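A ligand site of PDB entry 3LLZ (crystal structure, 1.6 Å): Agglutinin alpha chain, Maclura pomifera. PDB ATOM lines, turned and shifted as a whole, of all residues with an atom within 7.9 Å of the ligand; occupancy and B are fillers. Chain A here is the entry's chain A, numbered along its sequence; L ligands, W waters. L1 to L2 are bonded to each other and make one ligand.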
ATOM      1  N   GLY A   1     -17.749 -26.756   8.063  1.00  0.00           N
ATOM      2  CA  GLY A   1     -16.527 -27.526   8.436  1.00  0.00           C
ATOM      3  C   GLY A   1     -16.141 -28.515   7.354  1.00  0.00           C
ATOM      4  O   GLY A   1     -16.769 -28.579   6.298  1.00  0.00           O
ATOM      5  N   VAL A   2     -15.082 -29.289   7.617  1.00  0.00           N
ATOM      6  CA  VAL A   2     -14.641 -30.293   6.672  1.00  0.00           C
ATOM      7  C   VAL A   2     -15.473 -31.545   6.923  1.00  0.00           C
ATOM      8  O   VAL A   2     -15.499 -32.061   8.043  1.00  0.00           O
ATOM      9  CB  VAL A   2     -13.144 -30.621   6.866  1.00  0.00           C
ATOM     10  CG1 VAL A   2     -12.739 -31.776   5.950  1.00  0.00           C
ATOM     11  CG2 VAL A   2     -12.298 -29.384   6.567  1.00  0.00           C
ATOM     12  N   THR A   3     -16.155 -32.027   5.887  1.00  0.00           N
ATOM     13  CA  THR A   3     -16.969 -33.221   6.041  1.00  0.00           C
ATOM     14  C   THR A   3     -16.105 -34.465   6.074  1.00  0.00           C
ATOM     15  O   THR A   3     -15.012 -34.508   5.506  1.00  0.00           O
ATOM     16  CB  THR A   3     -17.976 -33.373   4.868  1.00  0.00           C
ATOM     17  OG1 THR A   3     -17.257 -33.430   3.632  1.00  0.00           O
ATOM     18  CG2 THR A   3     -18.938 -32.195   4.844  1.00  0.00           C
ATOM     19  N   ILE A  25     -18.345 -29.545  21.308  1.00  0.00           N
ATOM     20  CA  ILE A  25     -17.496 -30.673  20.976  1.00  0.00           C
ATOM     21  C   ILE A  25     -16.532 -30.256  19.871  1.00  0.00           C
ATOM     22  O   ILE A  25     -16.904 -29.503  18.970  1.00  0.00           O
ATOM     23  CB  ILE A  25     -18.346 -31.880  20.472  1.00  0.00           C
ATOM     24  CG1 ILE A  25     -19.337 -32.312  21.571  1.00  0.00           C
ATOM     25  CG2 ILE A  25     -17.437 -33.043  20.085  1.00  0.00           C
ATOM     26  CD1 ILE A  25     -18.683 -32.705  22.883  1.00  0.00           C
ATOM     27  N   SER A  46     -10.429 -30.390  14.837  1.00  0.00           N
ATOM     28  CA  SER A  46     -11.116 -29.118  14.975  1.00  0.00           C
ATOM     29  C   SER A  46     -10.182 -28.111  14.316  1.00  0.00           C
ATOM     30  O   SER A  46      -8.972 -28.350  14.215  1.00  0.00           O
ATOM     31  CB  SER A  46     -11.289 -28.766  16.447  1.00  0.00           C
ATOM     32  OG  SER A  46     -11.552 -27.374  16.598  1.00  0.00           O
ATOM     33  N   PHE A  47     -10.729 -26.980  13.869  1.00  0.00           N
ATOM     34  CA  PHE A  47      -9.928 -25.936  13.254  1.00  0.00           C
ATOM     35  C   PHE A  47      -9.123 -25.195  14.315  1.00  0.00           C
ATOM     36  O   PHE A  47      -8.215 -24.432  13.996  1.00  0.00           O
ATOM     37  CB  PHE A  47     -10.817 -24.917  12.537  1.00  0.00           C
ATOM     38  CG  PHE A  47     -11.435 -25.405  11.237  1.00  0.00           C
ATOM     39  CD1 PHE A  47     -12.213 -24.545  10.487  1.00  0.00           C
ATOM     40  CD2 PHE A  47     -11.243 -26.706  10.796  1.00  0.00           C
ATOM     41  CE1 PHE A  47     -12.806 -24.965   9.298  1.00  0.00           C
ATOM     42  CE2 PHE A  47     -11.831 -27.148   9.605  1.00  0.00           C
ATOM     43  CZ  PHE A  47     -12.613 -26.275   8.852  1.00  0.00           C
ATOM     44  N   ILE A  48      -9.466 -25.420  15.580  1.00  0.00           N
ATOM     45  CA  ILE A  48      -8.787 -24.758  16.695  1.00  0.00           C
ATOM     46  C   ILE A  48      -8.384 -25.688  17.837  1.00  0.00           C
ATOM     47  O   ILE A  48      -8.639 -26.893  17.807  1.00  0.00           O
ATOM     48  CB  ILE A  48      -9.675 -23.641  17.288  1.00  0.00           C
ATOM     49  CG1 ILE A  48     -11.006 -24.230  17.743  1.00  0.00           C
ATOM     50  CG2 ILE A  48      -9.900 -22.556  16.253  1.00  0.00           C
ATOM     51  CD1 ILE A  48     -11.849 -23.262  18.558  1.00  0.00           C
ATOM     52  N   VAL A  75     -22.970 -21.710  18.862  1.00  0.00           N
ATOM     53  CA  VAL A  75     -21.715 -21.209  19.398  1.00  0.00           C
ATOM     54  C   VAL A  75     -21.235 -20.276  18.296  1.00  0.00           C
ATOM     55  O   VAL A  75     -21.023 -20.707  17.161  1.00  0.00           O
ATOM     56  CB  VAL A  75     -20.694 -22.341  19.632  1.00  0.00           C
ATOM     57  CG1 VAL A  75     -19.376 -21.758  20.103  1.00  0.00           C
ATOM     58  CG2 VAL A  75     -21.235 -23.319  20.668  1.00  0.00           C
ATOM     59  N   GLU A  76     -21.090 -19.001  18.624  1.00  0.00           N
ATOM     60  CA  GLU A  76     -20.666 -18.007  17.651  1.00  0.00           C
ATOM     61  C   GLU A  76     -21.589 -18.036  16.434  1.00  0.00           C
ATOM     62  O   GLU A  76     -21.153 -17.818  15.306  1.00  0.00           O
ATOM     63  CB  GLU A  76     -19.200 -18.235  17.258  1.00  0.00           C
ATOM     64  CG  GLU A  76     -18.218 -17.765  18.313  1.00  0.00           C
ATOM     65  CD  GLU A  76     -16.791 -18.217  18.059  1.00  0.00           C
ATOM     66  OE1 GLU A  76     -16.356 -18.253  16.889  1.00  0.00           O
ATOM     67  OE2 GLU A  76     -16.084 -18.528  19.045  1.00  0.00           O
ATOM     68  N   GLY A  77     -22.871 -18.312  16.675  1.00  0.00           N
ATOM     69  CA  GLY A  77     -23.845 -18.346  15.594  1.00  0.00           C
ATOM     70  C   GLY A  77     -23.973 -19.641  14.823  1.00  0.00           C
ATOM     71  O   GLY A  77     -24.925 -19.815  14.055  1.00  0.00           O
ATOM     72  N   TYR A  78     -23.014 -20.554  15.001  1.00  0.00           N
ATOM     73  CA  TYR A  78     -23.054 -21.833  14.311  1.00  0.00           C
ATOM     74  C   TYR A  78     -23.770 -22.893  15.130  1.00  0.00           C
ATOM     75  O   TYR A  78     -23.537 -23.027  16.321  1.00  0.00           O
ATOM     76  CB  TYR A  78     -21.620 -22.315  14.013  1.00  0.00           C
ATOM     77  CG  TYR A  78     -20.920 -21.525  12.931  1.00  0.00           C
ATOM     78  CD1 TYR A  78     -20.000 -20.526  13.258  1.00  0.00           C
ATOM     79  CD2 TYR A  78     -21.162 -21.778  11.582  1.00  0.00           C
ATOM     80  CE1 TYR A  78     -19.346 -19.802  12.260  1.00  0.00           C
ATOM     81  CE2 TYR A  78     -20.518 -21.057  10.584  1.00  0.00           C
ATOM     82  CZ  TYR A  78     -19.612 -20.081  10.922  1.00  0.00           C
ATOM     83  OH  TYR A  78     -18.962 -19.387   9.930  1.00  0.00           O
ATOM     84  N   THR A  79     -24.654 -23.652  14.473  1.00  0.00           N
ATOM     85  CA  THR A  79     -25.391 -24.708  15.167  1.00  0.00           C
ATOM     86  C   THR A  79     -24.482 -25.924  15.210  1.00  0.00           C
ATOM     87  O   THR A  79     -24.136 -26.488  14.175  1.00  0.00           O
ATOM     88  CB  THR A  79     -26.690 -25.066  14.418  1.00  0.00           C
ATOM     89  OG1 THR A  79     -27.513 -23.904  14.304  1.00  0.00           O
ATOM     90  CG2 THR A  79     -27.451 -26.149  15.182  1.00  0.00           C
ATOM     91  N   VAL A  80     -24.084 -26.320  16.414  1.00  0.00           N
ATOM     92  CA  VAL A  80     -23.170 -27.433  16.581  1.00  0.00           C
ATOM     93  C   VAL A  80     -23.557 -28.370  17.703  1.00  0.00           C
ATOM     94  O   VAL A  80     -24.486 -28.111  18.466  1.00  0.00           O
ATOM     95  CB  VAL A  80     -21.743 -26.913  16.854  1.00  0.00           C
ATOM     96  CG1 VAL A  80     -21.249 -26.079  15.687  1.00  0.00           C
ATOM     97  CG2 VAL A  80     -21.734 -26.075  18.141  1.00  0.00           C
ATOM     98  N   ILE A  81     -22.836 -29.488  17.788  1.00  0.00           N
ATOM     99  CA  ILE A  81     -23.070 -30.461  18.854  1.00  0.00           C
ATOM    100  C   ILE A  81     -22.287 -29.934  20.045  1.00  0.00           C
ATOM    101  O   ILE A  81     -21.053 -29.890  20.024  1.00  0.00           O
ATOM    102  CB  ILE A  81     -22.565 -31.872  18.453  1.00  0.00           C
ATOM    103  CG1 ILE A  81     -23.366 -32.411  17.255  1.00  0.00           C
ATOM    104  CG2 ILE A  81     -22.730 -32.834  19.621  1.00  0.00           C
ATOM    105  CD1 ILE A  81     -23.261 -31.583  16.010  1.00  0.00           C
ATOM    106  N   SER A 119     -19.301 -33.612  10.075  1.00  0.00           N
ATOM    107  CA  SER A 119     -18.554 -32.432   9.660  1.00  0.00           C
ATOM    108  C   SER A 119     -17.985 -31.738  10.870  1.00  0.00           C
ATOM    109  O   SER A 119     -18.656 -31.621  11.887  1.00  0.00           O
ATOM    110  CB  SER A 119     -19.482 -31.466   8.916  1.00  0.00           C
ATOM    111  OG  SER A 119     -18.855 -30.215   8.681  1.00  0.00           O
ATOM    112  N   ILE A 120     -16.735 -31.288  10.779  1.00  0.00           N
ATOM    113  CA  ILE A 120     -16.118 -30.584  11.881  1.00  0.00           C
ATOM    114  C   ILE A 120     -15.360 -29.360  11.385  1.00  0.00           C
ATOM    115  O   ILE A 120     -14.554 -29.446  10.464  1.00  0.00           O
ATOM    116  CB  ILE A 120     -15.124 -31.482  12.659  1.00  0.00           C
ATOM    117  CG1 ILE A 120     -15.836 -32.765  13.112  1.00  0.00           C
ATOM    118  CG2 ILE A 120     -14.581 -30.726  13.876  1.00  0.00           C
ATOM    119  CD1 ILE A 120     -14.959 -33.693  13.947  1.00  0.00           C
ATOM    120  N   GLY A 121     -15.669 -28.215  11.983  1.00  0.00           N
ATOM    121  CA  GLY A 121     -15.002 -26.962  11.649  1.00  0.00           C
ATOM    122  C   GLY A 121     -14.357 -26.589  12.967  1.00  0.00           C
ATOM    123  O   GLY A 121     -13.515 -27.318  13.469  1.00  0.00           O
ATOM    124  N   TYR A 122     -14.745 -25.456  13.534  1.00  0.00           N
ATOM    125  CA  TYR A 122     -14.212 -25.085  14.831  1.00  0.00           C
ATOM    126  C   TYR A 122     -14.758 -26.128  15.814  1.00  0.00           C
ATOM    127  O   TYR A 122     -14.072 -26.522  16.752  1.00  0.00           O
ATOM    128  CB  TYR A 122     -14.694 -23.686  15.221  1.00  0.00           C
ATOM    129  CG  TYR A 122     -13.816 -22.579  14.669  1.00  0.00           C
ATOM    130  CD1 TYR A 122     -13.575 -22.483  13.302  1.00  0.00           C
ATOM    131  CD2 TYR A 122     -13.208 -21.658  15.516  1.00  0.00           C
ATOM    132  CE1 TYR A 122     -12.740 -21.497  12.788  1.00  0.00           C
ATOM    133  CE2 TYR A 122     -12.363 -20.668  15.015  1.00  0.00           C
ATOM    134  CZ  TYR A 122     -12.137 -20.598  13.646  1.00  0.00           C
ATOM    135  OH  TYR A 122     -11.288 -19.626  13.157  1.00  0.00           O
ATOM    136  N   TRP A 123     -15.977 -26.573  15.559  1.00  0.00           N
ATOM    137  CA  TRP A 123     -16.635 -27.576  16.405  1.00  0.00           C
ATOM    138  C   TRP A 123     -17.327 -28.617  15.543  1.00  0.00           C
ATOM    139  O   TRP A 123     -17.426 -28.480  14.322  1.00  0.00           O
ATOM    140  CB  TRP A 123     -17.659 -26.884  17.311  1.00  0.00           C
ATOM    141  CG  TRP A 123     -17.041 -25.787  18.100  1.00  0.00           C
ATOM    142  CD1 TRP A 123     -16.174 -25.908  19.134  1.00  0.00           C
ATOM    143  CD2 TRP A 123     -17.142 -24.378  17.821  1.00  0.00           C
ATOM    144  NE1 TRP A 123     -15.710 -24.678  19.518  1.00  0.00           N
ATOM    145  CE2 TRP A 123     -16.286 -23.719  18.729  1.00  0.00           C
ATOM    146  CE3 TRP A 123     -17.865 -23.619  16.893  1.00  0.00           C
ATOM    147  CZ2 TRP A 123     -16.127 -22.326  18.736  1.00  0.00           C
ATOM    148  CZ3 TRP A 123     -17.704 -22.234  16.894  1.00  0.00           C
ATOM    149  CH2 TRP A 123     -16.840 -21.607  17.816  1.00  0.00           C
ATOM    150  N   LEU A 124     -17.807 -29.672  16.199  1.00  0.00           N
ATOM    151  CA  LEU A 124     -18.535 -30.736  15.506  1.00  0.00           C
ATOM    152  C   LEU A 124     -19.851 -30.133  15.019  1.00  0.00           C
ATOM    153  O   LEU A 124     -20.729 -29.829  15.826  1.00  0.00           O
ATOM    154  CB  LEU A 124     -18.789 -31.883  16.477  1.00  0.00           C
ATOM    155  CG  LEU A 124     -19.612 -33.070  15.971  1.00  0.00           C
ATOM    156  CD1 LEU A 124     -18.954 -33.690  14.748  1.00  0.00           C
ATOM    157  CD2 LEU A 124     -19.752 -34.096  17.096  1.00  0.00           C
ATOM    158  N   ASP A 125     -19.972 -29.945  13.715  1.00  0.00           N
ATOM    159  CA  ASP A 125     -21.173 -29.341  13.139  1.00  0.00           C
ATOM    160  C   ASP A 125     -22.385 -30.250  13.234  1.00  0.00           C
ATOM    161  O   ASP A 125     -23.490 -29.810  13.588  1.00  0.00           O
ATOM    162  CB  ASP A 125     -20.932 -28.989  11.683  1.00  0.00           C
ATOM    163  CG  ASP A 125     -19.740 -28.084  11.494  1.00  0.00           C
ATOM    164  OD1 ASP A 125     -19.717 -26.991  12.106  1.00  0.00           O
ATOM    165  OD2 ASP A 125     -18.831 -28.469  10.727  1.00  0.00           O
ATOM    166  N   TYR A 126     -22.185 -31.505  12.892  1.00  0.00           N
ATOM    167  CA  TYR A 126     -23.256 -32.486  12.908  1.00  0.00           C
ATOM    168  C   TYR A 126     -22.620 -33.843  12.676  1.00  0.00           C
ATOM    169  O   TYR A 126     -21.453 -33.943  12.312  1.00  0.00           O
ATOM    170  CB  TYR A 126     -24.275 -32.203  11.795  1.00  0.00           C
ATOM    171  CG  TYR A 126     -23.691 -32.122  10.392  1.00  0.00           C
ATOM    172  CD1 TYR A 126     -23.452 -30.882   9.791  1.00  0.00           C
ATOM    173  CD2 TYR A 126     -23.391 -33.274   9.672  1.00  0.00           C
ATOM    174  CE1 TYR A 126     -22.920 -30.803   8.502  1.00  0.00           C
ATOM    175  CE2 TYR A 126     -22.867 -33.205   8.377  1.00  0.00           C
ATOM    176  CZ  TYR A 126     -22.628 -31.959   7.804  1.00  0.00           C
ATOM    177  OH  TYR A 126     -22.104 -31.893   6.532  1.00  0.00           O
HETATM  178  C1  LIG L   1     -16.065 -22.939  10.512  1.00  0.00           C
HETATM  179  C2  LIG L   1     -16.605 -23.619   9.236  1.00  0.00           C
HETATM  180  C3  LIG L   1     -18.126 -23.541   9.281  1.00  0.00           C
HETATM  181  C4  LIG L   1     -18.623 -24.280  10.544  1.00  0.00           C
HETATM  182  C5  LIG L   1     -18.007 -23.571  11.768  1.00  0.00           C
HETATM  183  C6  LIG L   1     -18.414 -24.172  13.115  1.00  0.00           C
HETATM  184  C7  LIG L   1     -15.577 -23.663   7.059  1.00  0.00           C
HETATM  185  C8  LIG L   1     -14.985 -22.894   5.896  1.00  0.00           C
HETATM  186  N1  LIG L   1     -16.103 -22.949   8.060  1.00  0.00           N
HETATM  187  O1  LIG L   1     -14.679 -23.014  10.524  1.00  0.00           O
HETATM  188  O2  LIG L   1     -18.746 -24.062   8.068  1.00  0.00           O
HETATM  189  O3  LIG L   1     -18.205 -25.632  10.502  1.00  0.00           O
HETATM  190  O4  LIG L   1     -16.563 -23.585  11.691  1.00  0.00           O
HETATM  191  O5  LIG L   1     -17.776 -25.421  13.368  1.00  0.00           O
HETATM  192  O6  LIG L   1     -15.559 -24.894   7.056  1.00  0.00           O
HETATM  193  C1  LG2 L   2     -19.620 -23.111   7.532  1.00  0.00           C
HETATM  194  C2  LG2 L   2     -19.534 -24.043   6.292  1.00  0.00           C
HETATM  195  C3  LG2 L   2     -20.673 -23.735   5.319  1.00  0.00           C
HETATM  196  C4  LG2 L   2     -22.043 -23.653   6.023  1.00  0.00           C
HETATM  197  C5  LG2 L   2     -21.961 -22.821   7.307  1.00  0.00           C
HETATM  198  C6  LG2 L   2     -23.236 -22.883   8.133  1.00  0.00           C
HETATM  199  O1  LG2 L   2     -18.289 -23.862   5.628  1.00  0.00           O
HETATM  200  O2  LG2 L   2     -20.733 -24.707   4.289  1.00  0.00           O
HETATM  201  O3  LG2 L   2     -22.512 -24.962   6.328  1.00  0.00           O
HETATM  202  O4  LG2 L   2     -20.893 -23.302   8.146  1.00  0.00           O
HETATM  203  O5  LG2 L   2     -24.146 -21.867   7.726  1.00  0.00           O
HETATM  204  O   HOH W   1     -21.674 -26.807   3.178  1.00  0.00           O
HETATM  205  O   HOH W   2     -17.679 -26.377   4.400  1.00  0.00           O
HETATM  206  O   HOH W   3     -22.002 -26.782   8.204  1.00  0.00           O
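The backbone NH (N) of Gly 1 sits at hydrogen-bond distance from an oxygen (O3) of LIG L1 (2.7 Å). The backbone NH of Tyr 122 sits at hydrogen-bond distance from an oxygen (O5) of LIG L1, 3.0 Å away. O5 of LIG L1 is in hydrogen-bond range of N of Trp 123 (3.1 Å). The backbone carbonyl oxygen (O) of Trp 123 lies within hydrogen-bond range of an oxygen (O5) of LIG L1 (3.2 Å). O3 of LIG L1 is in hydrogen-bond range of OD1 of Asp 125 (2.6 Å).
OD2 of Asp 125 lies within hydrogen-bond range of N of Gly 121, at 3.4 Å. The side-chain carboxylate (OD2) of Asp 125 sits at hydrogen-bond distance from the side-chain hydroxyl (OG) of Ser 119, 2.7 Å away. The backbone NH (N) of Phe 47 is in hydrogen-bond range of the backbone carbonyl oxygen (O) of Gly 121 (2.8 Å). N of Gly 1 lies within hydrogen-bond range of OD2 of Asp 125, at 3.3 Å. O of Tyr 122 is in hydrogen-bond range of OG of Ser 46 (2.7 Å).
Phe 47 touches the ligand. Tyr 78 touches the ligand. CA of Gly 121 touches O5 of LIG L1, at 3.6 Å. Hydrophobic or aromatic side chains that line the ligand: Phe 47, Tyr 78, Tyr 122 and Trp 123.
Water W2 lies within hydrogen-bond range of O1 of LG2 L2 (2.9 Å) and O of Gly 1 (3.0 Å).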
